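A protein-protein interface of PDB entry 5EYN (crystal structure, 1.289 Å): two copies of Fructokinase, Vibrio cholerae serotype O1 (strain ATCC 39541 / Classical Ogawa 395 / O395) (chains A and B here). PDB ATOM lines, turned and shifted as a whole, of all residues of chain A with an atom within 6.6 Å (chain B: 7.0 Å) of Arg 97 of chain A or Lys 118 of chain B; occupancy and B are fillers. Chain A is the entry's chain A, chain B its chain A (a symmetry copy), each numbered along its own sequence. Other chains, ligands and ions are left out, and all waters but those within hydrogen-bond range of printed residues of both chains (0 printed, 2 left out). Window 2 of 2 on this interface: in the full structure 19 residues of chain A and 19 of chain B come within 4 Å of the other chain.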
ATOM      1  N   VAL A  67     -23.715 -29.648  11.062  1.00  0.00           N
ATOM      2  CA  VAL A  67     -23.385 -28.249  10.836  1.00  0.00           C
ATOM      3  C   VAL A  67     -24.583 -27.564  10.198  1.00  0.00           C
ATOM      4  O   VAL A  67     -25.615 -28.188   9.975  1.00  0.00           O
ATOM      5  CB  VAL A  67     -22.154 -28.091   9.931  1.00  0.00           C
ATOM      6  CG1 VAL A  67     -20.898 -28.549  10.666  1.00  0.00           C
ATOM      7  CG2 VAL A  67     -22.346 -28.833   8.607  1.00  0.00           C
ATOM      8  N   GLY A  68     -24.467 -26.271   9.938  1.00  0.00           N
ATOM      9  CA  GLY A  68     -25.557 -25.558   9.318  1.00  0.00           C
ATOM     10  C   GLY A  68     -25.509 -25.615   7.810  1.00  0.00           C
ATOM     11  O   GLY A  68     -24.452 -25.840   7.223  1.00  0.00           O
ATOM     12  N   ASN A  69     -26.669 -25.412   7.198  1.00  0.00           N
ATOM     13  CA  ASN A  69     -26.782 -25.256   5.760  1.00  0.00           C
ATOM     14  C   ASN A  69     -26.415 -23.827   5.412  1.00  0.00           C
ATOM     15  O   ASN A  69     -27.280 -22.981   5.174  1.00  0.00           O
ATOM     16  CB  ASN A  69     -28.205 -25.570   5.315  1.00  0.00           C
ATOM     17  CG  ASN A  69     -28.348 -25.604   3.816  1.00  0.00           C
ATOM     18  OD1 ASN A  69     -27.364 -25.515   3.083  1.00  0.00           O
ATOM     19  ND2 ASN A  69     -29.583 -25.737   3.345  1.00  0.00           N
ATOM     20  N   ASP A  70     -25.114 -23.567   5.426  1.00  0.00           N
ATOM     21  CA  ASP A  70     -24.576 -22.237   5.209  1.00  0.00           C
ATOM     22  C   ASP A  70     -23.161 -22.404   4.688  1.00  0.00           C
ATOM     23  O   ASP A  70     -22.622 -23.518   4.682  1.00  0.00           O
ATOM     24  CB  ASP A  70     -24.614 -21.402   6.501  1.00  0.00           C
ATOM     25  CG  ASP A  70     -24.101 -22.156   7.707  1.00  0.00           C
ATOM     26  OD1 ASP A  70     -24.860 -22.282   8.693  1.00  0.00           O
ATOM     27  OD2 ASP A  70     -22.944 -22.614   7.686  1.00  0.00           O
ATOM     28  N   PRO A  71     -22.557 -21.306   4.220  1.00  0.00           N
ATOM     29  CA  PRO A  71     -21.228 -21.446   3.619  1.00  0.00           C
ATOM     30  C   PRO A  71     -20.213 -22.031   4.592  1.00  0.00           C
ATOM     31  O   PRO A  71     -19.349 -22.783   4.175  1.00  0.00           O
ATOM     32  CB  PRO A  71     -20.878 -20.004   3.223  1.00  0.00           C
ATOM     33  CG  PRO A  71     -22.192 -19.389   2.924  1.00  0.00           C
ATOM     34  CD  PRO A  71     -23.128 -19.968   3.970  1.00  0.00           C
ATOM     35  N   ASP A  93     -28.113 -29.333   9.424  1.00  0.00           N
ATOM     36  CA  ASP A  93     -29.355 -29.016  10.116  1.00  0.00           C
ATOM     37  C   ASP A  93     -30.173 -28.068   9.256  1.00  0.00           C
ATOM     38  O   ASP A  93     -29.616 -27.161   8.623  1.00  0.00           O
ATOM     39  CB  ASP A  93     -29.078 -28.357  11.464  1.00  0.00           C
ATOM     40  CG  ASP A  93     -30.324 -28.226  12.305  1.00  0.00           C
ATOM     41  OD1 ASP A  93     -30.670 -29.206  12.991  1.00  0.00           O
ATOM     42  OD2 ASP A  93     -30.966 -27.155  12.275  1.00  0.00           O
ATOM     43  N   PRO A  94     -31.495 -28.267   9.229  1.00  0.00           N
ATOM     44  CA  PRO A  94     -32.330 -27.427   8.363  1.00  0.00           C
ATOM     45  C   PRO A  94     -32.458 -25.968   8.809  1.00  0.00           C
ATOM     46  O   PRO A  94     -32.768 -25.113   7.984  1.00  0.00           O
ATOM     47  CB  PRO A  94     -33.696 -28.129   8.407  1.00  0.00           C
ATOM     48  CG  PRO A  94     -33.670 -28.965   9.632  1.00  0.00           C
ATOM     49  CD  PRO A  94     -32.258 -29.378   9.832  1.00  0.00           C
ATOM     50  N   VAL A  95     -32.208 -25.685  10.080  1.00  0.00           N
ATOM     51  CA  VAL A  95     -32.552 -24.383  10.645  1.00  0.00           C
ATOM     52  C   VAL A  95     -31.360 -23.637  11.246  1.00  0.00           C
ATOM     53  O   VAL A  95     -31.212 -22.434  11.070  1.00  0.00           O
ATOM     54  CB  VAL A  95     -33.649 -24.558  11.734  1.00  0.00           C
ATOM     55  CG1 VAL A  95     -33.812 -23.287  12.569  1.00  0.00           C
ATOM     56  CG2 VAL A  95     -34.970 -24.974  11.098  1.00  0.00           C
ATOM     57  N   HIS A  96     -30.515 -24.348  11.967  1.00  0.00           N
ATOM     58  CA  HIS A  96     -29.501 -23.707  12.785  1.00  0.00           C
ATOM     59  C   HIS A  96     -28.176 -23.533  12.054  1.00  0.00           C
ATOM     60  O   HIS A  96     -27.842 -24.294  11.167  1.00  0.00           O
ATOM     61  CB  HIS A  96     -29.337 -24.508  14.072  1.00  0.00           C
ATOM     62  CG  HIS A  96     -30.609 -24.622  14.841  1.00  0.00           C
ATOM     63  ND1 HIS A  96     -31.086 -23.593  15.620  1.00  0.00           N
ATOM     64  CD2 HIS A  96     -31.522 -25.619  14.923  1.00  0.00           C
ATOM     65  CE1 HIS A  96     -32.240 -23.954  16.155  1.00  0.00           C
ATOM     66  NE2 HIS A  96     -32.521 -25.183  15.756  1.00  0.00           N
ATOM     67  N   ARG A  97     -27.429 -22.520  12.460  1.00  0.00           N
ATOM     68  CA  ARG A  97     -26.207 -22.117  11.808  1.00  0.00           C
ATOM     69  C   ARG A  97     -24.978 -22.826  12.364  1.00  0.00           C
ATOM     70  O   ARG A  97     -24.932 -23.249  13.514  1.00  0.00           O
ATOM     71  CB  ARG A  97     -26.054 -20.606  11.971  1.00  0.00           C
ATOM     72  CG  ARG A  97     -27.027 -19.820  11.099  1.00  0.00           C
ATOM     73  CD  ARG A  97     -26.410 -19.625   9.743  1.00  0.00           C
ATOM     74  NE  ARG A  97     -27.357 -19.155   8.760  1.00  0.00           N
ATOM     75  CZ  ARG A  97     -28.025 -19.935   7.928  1.00  0.00           C
ATOM     76  NH1 ARG A  97     -27.867 -21.252   7.962  1.00  0.00           N
ATOM     77  NH2 ARG A  97     -28.867 -19.392   7.060  1.00  0.00           N
ATOM     78  N   THR A  98     -23.971 -22.944  11.513  1.00  0.00           N
ATOM     79  CA  THR A  98     -22.666 -23.461  11.896  1.00  0.00           C
ATOM     80  C   THR A  98     -21.982 -22.597  12.934  1.00  0.00           C
ATOM     81  O   THR A  98     -21.987 -21.362  12.862  1.00  0.00           O
ATOM     82  CB  THR A  98     -21.770 -23.560  10.668  1.00  0.00           C
ATOM     83  OG1 THR A  98     -22.426 -24.357   9.689  1.00  0.00           O
ATOM     84  CG2 THR A  98     -20.412 -24.161  11.002  1.00  0.00           C
ATOM     85  N   SER A  99     -21.397 -23.260  13.918  1.00  0.00           N
ATOM     86  CA  SER A  99     -20.655 -22.568  14.949  1.00  0.00           C
ATOM     87  C   SER A  99     -19.563 -21.680  14.342  1.00  0.00           C
ATOM     88  O   SER A  99     -18.812 -22.102  13.462  1.00  0.00           O
ATOM     89  CB  SER A  99     -20.025 -23.573  15.895  1.00  0.00           C
ATOM     90  OG  SER A  99     -19.335 -22.901  16.930  1.00  0.00           O
ATOM     91  N   THR A 100     -19.489 -20.462  14.856  1.00  0.00           N
ATOM     92  CA  THR A 100     -18.556 -19.437  14.421  1.00  0.00           C
ATOM     93  C   THR A 100     -17.906 -18.860  15.652  1.00  0.00           C
ATOM     94  O   THR A 100     -18.584 -18.330  16.523  1.00  0.00           O
ATOM     95  CB  THR A 100     -19.291 -18.340  13.656  1.00  0.00           C
ATOM     96  OG1 THR A 100     -19.970 -18.921  12.552  1.00  0.00           O
ATOM     97  CG2 THR A 100     -18.330 -17.293  13.135  1.00  0.00           C
ATOM     98  N   MET A 116     -19.998 -17.137  18.728  1.00  0.00           N
ATOM     99  CA  MET A 116     -21.007 -16.237  18.194  1.00  0.00           C
ATOM    100  C   MET A 116     -22.350 -16.896  17.918  1.00  0.00           C
ATOM    101  O   MET A 116     -23.368 -16.202  17.854  1.00  0.00           O
ATOM    102  CB  MET A 116     -20.515 -15.540  16.930  1.00  0.00           C
ATOM    103  CG  MET A 116     -19.285 -14.692  17.135  1.00  0.00           C
ATOM    104  SD  MET A 116     -19.435 -13.454  18.418  1.00  0.00           S
ATOM    105  CE  MET A 116     -20.712 -12.403  17.712  1.00  0.00           C
ATOM    106  N   VAL A 117     -22.356 -18.215  17.752  1.00  0.00           N
ATOM    107  CA  VAL A 117     -23.578 -18.936  17.403  1.00  0.00           C
ATOM    108  C   VAL A 117     -23.916 -19.896  18.531  1.00  0.00           C
ATOM    109  O   VAL A 117     -23.247 -20.915  18.730  1.00  0.00           O
ATOM    110  CB  VAL A 117     -23.430 -19.691  16.063  1.00  0.00           C
ATOM    111  CG1 VAL A 117     -24.732 -20.371  15.689  1.00  0.00           C
ATOM    112  CG2 VAL A 117     -22.995 -18.750  14.953  1.00  0.00           C
ATOM    113  N   LYS A 118     -24.982 -19.564  19.253  1.00  0.00           N
ATOM    114  CA  LYS A 118     -25.418 -20.307  20.422  1.00  0.00           C
ATOM    115  C   LYS A 118     -26.940 -20.320  20.423  1.00  0.00           C
ATOM    116  O   LYS A 118     -27.551 -19.286  20.571  1.00  0.00           O
ATOM    117  CB  LYS A 118     -24.927 -19.614  21.695  1.00  0.00           C
ATOM    118  CG  LYS A 118     -23.403 -19.581  21.811  1.00  0.00           C
ATOM    119  CD  LYS A 118     -22.931 -19.205  23.206  1.00  0.00           C
ATOM    120  CE  LYS A 118     -23.475 -17.873  23.647  1.00  0.00           C
ATOM    121  NZ  LYS A 118     -22.912 -17.482  24.966  1.00  0.00           N
ATOM    122  N   PRO A 119     -27.561 -21.492  20.257  1.00  0.00           N
ATOM    123  CA  PRO A 119     -26.982 -22.813  19.998  1.00  0.00           C
ATOM    124  C   PRO A 119     -26.703 -23.021  18.505  1.00  0.00           C
ATOM    125  O   PRO A 119     -27.574 -22.777  17.675  1.00  0.00           O
ATOM    126  CB  PRO A 119     -28.088 -23.758  20.490  1.00  0.00           C
ATOM    127  CG  PRO A 119     -29.349 -22.999  20.208  1.00  0.00           C
ATOM    128  CD  PRO A 119     -29.027 -21.561  20.442  1.00  0.00           C
ATOM    129  N   SER A 120     -25.513 -23.505  18.176  1.00  0.00           N
ATOM    130  CA  SER A 120     -25.207 -23.828  16.794  1.00  0.00           C
ATOM    131  C   SER A 120     -25.779 -25.198  16.412  1.00  0.00           C
ATOM    132  O   SER A 120     -26.320 -25.926  17.254  1.00  0.00           O
ATOM    133  CB  SER A 120     -23.695 -23.785  16.576  1.00  0.00           C
ATOM    134  OG  SER A 120     -23.026 -24.561  17.563  1.00  0.00           O
ATOM    135  N   ALA A 121     -25.666 -25.533  15.138  1.00  0.00           N
ATOM    136  CA  ALA A 121     -26.313 -26.703  14.583  1.00  0.00           C
ATOM    137  C   ALA A 121     -25.972 -27.999  15.309  1.00  0.00           C
ATOM    138  O   ALA A 121     -26.818 -28.882  15.448  1.00  0.00           O
ATOM    139  CB  ALA A 121     -25.939 -26.833  13.110  1.00  0.00           C
ATOM    140  N   ASP A 122     -24.723 -28.124  15.731  1.00  0.00           N
ATOM    141  CA  ASP A 122     -24.250 -29.331  16.397  1.00  0.00           C
ATOM    142  C   ASP A 122     -25.000 -29.609  17.690  1.00  0.00           C
ATOM    143  O   ASP A 122     -25.070 -30.754  18.116  1.00  0.00           O
ATOM    144  CB  ASP A 122     -22.737 -29.216  16.667  1.00  0.00           C
ATOM    145  CG  ASP A 122     -22.376 -27.919  17.333  1.00  0.00           C
ATOM    146  OD1 ASP A 122     -22.184 -27.908  18.564  1.00  0.00           O
ATOM    147  OD2 ASP A 122     -22.309 -26.890  16.622  1.00  0.00           O
ATOM    148  N   ARG B  97     -25.954 -12.598  21.161  1.00  0.00           N
ATOM    149  CA  ARG B  97     -24.764 -12.176  20.464  1.00  0.00           C
ATOM    150  C   ARG B  97     -25.050 -11.144  19.379  1.00  0.00           C
ATOM    151  O   ARG B  97     -26.134 -11.077  18.810  1.00  0.00           O
ATOM    152  CB  ARG B  97     -24.108 -13.410  19.847  1.00  0.00           C
ATOM    153  CG  ARG B  97     -23.436 -14.300  20.888  1.00  0.00           C
ATOM    154  CD  ARG B  97     -22.037 -13.804  21.114  1.00  0.00           C
ATOM    155  NE  ARG B  97     -21.419 -14.387  22.282  1.00  0.00           N
ATOM    156  CZ  ARG B  97     -21.407 -13.831  23.481  1.00  0.00           C
ATOM    157  NH1 ARG B  97     -22.001 -12.663  23.692  1.00  0.00           N
ATOM    158  NH2 ARG B  97     -20.802 -14.455  24.482  1.00  0.00           N
ATOM    159  N   SER B  99     -25.049  -9.484  15.819  1.00  0.00           N
ATOM    160  CA  SER B  99     -25.229  -9.984  14.474  1.00  0.00           C
ATOM    161  C   SER B  99     -23.895 -10.041  13.722  1.00  0.00           C
ATOM    162  O   SER B  99     -23.109  -9.093  13.742  1.00  0.00           O
ATOM    163  CB  SER B  99     -26.200  -9.095  13.718  1.00  0.00           C
ATOM    164  OG  SER B  99     -26.414  -9.604  12.418  1.00  0.00           O
ATOM    165  N   THR B 114     -25.231 -13.838   4.389  1.00  0.00           N
ATOM    166  CA  THR B 114     -25.636 -14.956   5.223  1.00  0.00           C
ATOM    167  C   THR B 114     -25.572 -14.511   6.675  1.00  0.00           C
ATOM    168  O   THR B 114     -24.505 -14.111   7.163  1.00  0.00           O
ATOM    169  CB  THR B 114     -24.697 -16.161   5.052  1.00  0.00           C
ATOM    170  OG1 THR B 114     -24.671 -16.571   3.679  1.00  0.00           O
ATOM    171  CG2 THR B 114     -25.157 -17.335   5.918  1.00  0.00           C
ATOM    172  N   PHE B 115     -26.705 -14.578   7.364  1.00  0.00           N
ATOM    173  CA  PHE B 115     -26.790 -14.180   8.758  1.00  0.00           C
ATOM    174  C   PHE B 115     -26.443 -15.334   9.674  1.00  0.00           C
ATOM    175  O   PHE B 115     -27.158 -16.333   9.719  1.00  0.00           O
ATOM    176  CB  PHE B 115     -28.194 -13.640   9.047  1.00  0.00           C
ATOM    177  CG  PHE B 115     -28.437 -12.311   8.395  1.00  0.00           C
ATOM    178  CD1 PHE B 115     -28.329 -11.143   9.117  1.00  0.00           C
ATOM    179  CD2 PHE B 115     -28.681 -12.233   7.037  1.00  0.00           C
ATOM    180  CE1 PHE B 115     -28.485  -9.919   8.504  1.00  0.00           C
ATOM    181  CE2 PHE B 115     -28.842 -11.015   6.427  1.00  0.00           C
ATOM    182  CZ  PHE B 115     -28.741  -9.854   7.148  1.00  0.00           C
ATOM    183  N   MET B 116     -25.327 -15.223  10.382  1.00  0.00           N
ATOM    184  CA  MET B 116     -24.880 -16.316  11.230  1.00  0.00           C
ATOM    185  C   MET B 116     -25.513 -16.333  12.613  1.00  0.00           C
ATOM    186  O   MET B 116     -25.536 -17.383  13.260  1.00  0.00           O
ATOM    187  CB  MET B 116     -23.360 -16.324  11.368  1.00  0.00           C
ATOM    188  CG  MET B 116     -22.625 -16.499  10.064  1.00  0.00           C
ATOM    189  SD  MET B 116     -23.097 -17.950   9.128  1.00  0.00           S
ATOM    190  CE  MET B 116     -22.550 -19.250  10.242  1.00  0.00           C
ATOM    191  N   VAL B 117     -26.017 -15.188  13.065  1.00  0.00           N
ATOM    192  CA  VAL B 117     -26.575 -15.077  14.410  1.00  0.00           C
ATOM    193  C   VAL B 117     -28.052 -14.739  14.298  1.00  0.00           C
ATOM    194  O   VAL B 117     -28.429 -13.619  13.935  1.00  0.00           O
ATOM    195  CB  VAL B 117     -25.829 -14.016  15.250  1.00  0.00           C
ATOM    196  CG1 VAL B 117     -26.380 -13.970  16.661  1.00  0.00           C
ATOM    197  CG2 VAL B 117     -24.336 -14.297  15.281  1.00  0.00           C
ATOM    198  N   LYS B 118     -28.882 -15.720  14.638  1.00  0.00           N
ATOM    199  CA  LYS B 118     -30.326 -15.620  14.521  1.00  0.00           C
ATOM    200  C   LYS B 118     -30.939 -16.338  15.715  1.00  0.00           C
ATOM    201  O   LYS B 118     -30.803 -17.535  15.833  1.00  0.00           O
ATOM    202  CB  LYS B 118     -30.795 -16.305  13.236  1.00  0.00           C
ATOM    203  CG  LYS B 118     -30.264 -15.636  11.969  1.00  0.00           C
ATOM    204  CD  LYS B 118     -30.989 -16.098  10.715  1.00  0.00           C
ATOM    205  CE  LYS B 118     -30.912 -17.590  10.537  1.00  0.00           C
ATOM    206  NZ  LYS B 118     -31.533 -18.001   9.250  1.00  0.00           N
ATOM    207  N   PRO B 119     -31.617 -15.612  16.609  1.00  0.00           N
ATOM    208  CA  PRO B 119     -31.816 -14.160  16.655  1.00  0.00           C
ATOM    209  C   PRO B 119     -30.637 -13.452  17.331  1.00  0.00           C
ATOM    210  O   PRO B 119     -30.216 -13.851  18.414  1.00  0.00           O
ATOM    211  CB  PRO B 119     -33.094 -14.031  17.497  1.00  0.00           C
ATOM    212  CG  PRO B 119     -33.011 -15.193  18.440  1.00  0.00           C
ATOM    213  CD  PRO B 119     -32.378 -16.305  17.671  1.00  0.00           C
ATOM    214  N   SER B 120     -30.137 -12.390  16.715  1.00  0.00           N
ATOM    215  CA  SER B 120     -29.088 -11.603  17.338  1.00  0.00           C
ATOM    216  C   SER B 120     -29.672 -10.629  18.367  1.00  0.00           C
ATOM    217  O   SER B 120     -30.895 -10.505  18.513  1.00  0.00           O
ATOM    218  CB  SER B 120     -28.295 -10.857  16.266  1.00  0.00           C
ATOM    219  OG  SER B 120     -29.173 -10.152  15.395  1.00  0.00           O
ATOM    220  N   GLN B 123     -32.678  -8.209  18.038  1.00  0.00           N
ATOM    221  CA  GLN B 123     -34.022  -8.769  17.992  1.00  0.00           C
ATOM    222  C   GLN B 123     -34.730  -8.739  19.345  1.00  0.00           C
ATOM    223  O   GLN B 123     -35.939  -8.983  19.433  1.00  0.00           O
ATOM    224  CB  GLN B 123     -33.985 -10.202  17.440  1.00  0.00           C
ATOM    225  CG  GLN B 123     -33.493 -10.268  16.008  1.00  0.00           C
ATOM    226  CD  GLN B 123     -34.408  -9.526  15.069  1.00  0.00           C
ATOM    227  OE1 GLN B 123     -35.490  -9.995  14.768  1.00  0.00           O
ATOM    228  NE2 GLN B 123     -33.981  -8.355  14.600  1.00  0.00           N
ATOM    229  N   PHE B 124     -33.981  -8.385  20.384  1.00  0.00           N
ATOM    230  CA  PHE B 124     -34.506  -8.335  21.741  1.00  0.00           C
ATOM    231  C   PHE B 124     -34.698  -6.920  22.275  1.00  0.00           C
ATOM    232  O   PHE B 124     -34.851  -6.717  23.475  1.00  0.00           O
ATOM    233  CB  PHE B 124     -33.627  -9.194  22.648  1.00  0.00           C
ATOM    234  CG  PHE B 124     -33.673 -10.634  22.263  1.00  0.00           C
ATOM    235  CD1 PHE B 124     -32.785 -11.155  21.342  1.00  0.00           C
ATOM    236  CD2 PHE B 124     -34.663 -11.460  22.769  1.00  0.00           C
ATOM    237  CE1 PHE B 124     -32.862 -12.467  20.960  1.00  0.00           C
ATOM    238  CE2 PHE B 124     -34.743 -12.769  22.390  1.00  0.00           C
ATOM    239  CZ  PHE B 124     -33.839 -13.284  21.492  1.00  0.00           C
ATOM    240  N   ASN B 148     -38.545 -10.291  14.258  1.00  0.00           N
ATOM    241  CA  ASN B 148     -38.968 -11.158  15.351  1.00  0.00           C
ATOM    242  C   ASN B 148     -39.312 -10.332  16.560  1.00  0.00           C
ATOM    243  O   ASN B 148     -38.919  -9.179  16.666  1.00  0.00           O
ATOM    244  CB  ASN B 148     -37.867 -12.145  15.718  1.00  0.00           C
ATOM    245  CG  ASN B 148     -37.427 -12.971  14.544  1.00  0.00           C
ATOM    246  OD1 ASN B 148     -38.083 -13.942  14.154  1.00  0.00           O
ATOM    247  ND2 ASN B 148     -36.308 -12.597  13.971  1.00  0.00           N
ATOM    248  N   GLU B 177     -34.821 -11.838   4.224  1.00  0.00           N
ATOM    249  CA  GLU B 177     -35.863 -12.787   4.621  1.00  0.00           C
ATOM    250  C   GLU B 177     -35.377 -13.798   5.636  1.00  0.00           C
ATOM    251  O   GLU B 177     -36.139 -14.194   6.511  1.00  0.00           O
ATOM    252  CB  GLU B 177     -36.405 -13.535   3.396  1.00  0.00           C
ATOM    253  CG  GLU B 177     -37.587 -14.448   3.680  1.00  0.00           C
ATOM    254  CD  GLU B 177     -38.067 -15.133   2.420  1.00  0.00           C
ATOM    255  OE1 GLU B 177     -37.305 -15.946   1.856  1.00  0.00           O
ATOM    256  OE2 GLU B 177     -39.193 -14.835   1.979  1.00  0.00           O
ATOM    257  N   GLU B 178     -34.122 -14.238   5.531  1.00  0.00           N
ATOM    258  CA  GLU B 178     -33.689 -15.348   6.378  1.00  0.00           C
ATOM    259  C   GLU B 178     -33.658 -14.994   7.861  1.00  0.00           C
ATOM    260  O   GLU B 178     -33.624 -15.878   8.712  1.00  0.00           O
ATOM    261  CB  GLU B 178     -32.329 -15.892   5.960  1.00  0.00           C
ATOM    262  CG  GLU B 178     -31.152 -15.047   6.453  1.00  0.00           C
ATOM    263  CD  GLU B 178     -29.877 -15.882   6.586  1.00  0.00           C
ATOM    264  OE1 GLU B 178     -29.807 -16.853   7.399  1.00  0.00           O
ATOM    265  OE2 GLU B 178     -28.945 -15.587   5.857  1.00  0.00           O
ATOM    266  N   VAL B 179     -33.679 -13.707   8.175  1.00  0.00           N
ATOM    267  CA  VAL B 179     -33.664 -13.274   9.568  1.00  0.00           C
ATOM    268  C   VAL B 179     -35.014 -13.546  10.269  1.00  0.00           C
ATOM    269  O   VAL B 179     -35.083 -13.614  11.498  1.00  0.00           O
ATOM    270  CB  VAL B 179     -33.290 -11.763   9.616  1.00  0.00           C
ATOM    271  CG1 VAL B 179     -33.351 -11.185  11.018  1.00  0.00           C
ATOM    272  CG2 VAL B 179     -31.916 -11.569   9.027  1.00  0.00           C
ATOM    273  N   TRP B 180     -36.082 -13.682   9.492  1.00  0.00           N
ATOM    274  CA  TRP B 180     -37.431 -13.890  10.014  1.00  0.00           C
ATOM    275  C   TRP B 180     -37.618 -15.340  10.412  1.00  0.00           C
ATOM    276  O   TRP B 180     -37.463 -16.238   9.596  1.00  0.00           O
ATOM    277  CB  TRP B 180     -38.465 -13.519   8.939  1.00  0.00           C
ATOM    278  CG  TRP B 180     -38.423 -12.082   8.588  1.00  0.00           C
ATOM    279  CD1 TRP B 180     -37.399 -11.413   7.981  1.00  0.00           C
ATOM    280  CD2 TRP B 180     -39.420 -11.105   8.868  1.00  0.00           C
ATOM    281  NE1 TRP B 180     -37.708 -10.082   7.865  1.00  0.00           N
ATOM    282  CE2 TRP B 180     -38.938  -9.863   8.407  1.00  0.00           C
ATOM    283  CE3 TRP B 180     -40.677 -11.155   9.470  1.00  0.00           C
ATOM    284  CZ2 TRP B 180     -39.671  -8.690   8.516  1.00  0.00           C
ATOM    285  CZ3 TRP B 180     -41.410  -9.980   9.572  1.00  0.00           C
ATOM    286  CH2 TRP B 180     -40.900  -8.768   9.109  1.00  0.00           C
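N of Ala 121 of chain A is in hydrogen-bond range of O of Arg 97 of chain A, at 2.9 Å.
The backbone NH (N) of Met 116 of chain A lies within hydrogen-bond range of the backbone carbonyl oxygen (O) of Thr 100 of chain A (2.9 Å).
The side-chain hydroxyl (OG1) of Thr 98 of chain A sits at hydrogen-bond distance from the side-chain carboxylate (OD2) of Asp 70 of chain A, at 2.7 Å.
N of Phe 115 of chain B lies within hydrogen-bond range of OE2 of Glu 178 of chain B, 2.9 Å away.
The side-chain amino group (NZ) of Lys 118 of chain B lies within salt-bridge range of the side-chain carboxylate (OE1) of Glu 178 of chain B (2.8 Å).
The side-chain hydroxyl (OG1) of Thr 98 of chain A lies within hydrogen-bond range of the backbone NH (N) of Gly 68 of chain A, at 2.8 Å.
Among the printed residues, merely in contact across the chains: Pro 71 of chain A with Thr 114 of chain B (3.7 Å), Arg 97 of chain A with Met 116 of chain B (3.5 Å), Arg 97 of chain A with Lys 118 of chain B (3.7 Å), Thr 98 of chain A with Met 116 of chain B (3.4 Å), Thr 100 of chain A with Met 116 of chain B (3.5 Å), Met 116 of chain A with Arg 97 of chain B (3.5 Å), Met 116 of chain A with Val 117 of chain B (3.3 Å), Val 117 of chain A with Met 116 of chain B (3.3 Å) and Lys 118 of chain A with Arg 97 of chain B (3.7 Å).
The backbone carbonyl oxygen (O) of Phe 115 of chain B lies within hydrogen-bond range of the guanidinium group (NE) of Arg 97 of chain A, 3.0 Å away.
NH2 of Arg 97 of chain A is in salt-bridge range of OE1 of Glu 178 of chain B.
Of the 20 printed residues of chain A, 7 touch a printed residue of chain B.
Of the 16 printed residues of chain B, 7 touch a printed residue of chain A.
Among the printed residues, Asp or Glu carboxylates within 4 Å of a Lys or Arg side-chain nitrogen of the other chain: Arg 97 of chain A with Glu 178 of chain B (2.7 Å).
Arg 97 of chain A touches Met 116 of chain B, and with the chains exchanged Met 116 of chain A touches Arg 97 of chain B.
Arg 97 of chain A touches Lys 118 of chain B, and with the chains exchanged Lys 118 of chain A touches Arg 97 of chain B.
Met 116 of chain A touches Val 117 of chain B, and with the chains exchanged Val 117 of chain A touches Met 116 of chain B.
Positions printed for both chains: 97, 99, 116, 117, 118, 119 and 120.
Of the 11 pairs that touch across the chains among the printed residues, 6 have their exchanged pair printed and touching as well.
Printed residues of chain B within 4 Å of Pro 71 of chain A: Thr 114 (3.7 Å).
Of the printed residues of chain B, Thr 100 of chain A touches Met 116.
Of the printed residues of chain A, Arg 97 of chain B touches Met 116 (3.5 Å) and Lys 118 (3.7 Å).
Printed residues of chain A within 4 Å of Val 117 of chain B: Met 116 (3.3 Å).
Of chain A, only Arg 97 (3.7 Å) comes within 4 Å of Lys 118 of chain B.
The nearest residue of chain A that does not touch Lys 118 of chain B is Val 95 of chain A (4.8 Å).
The nearest printed residue of chain A that does not touch Arg 97 of chain B is Val 117 of chain A (5.1 Å).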
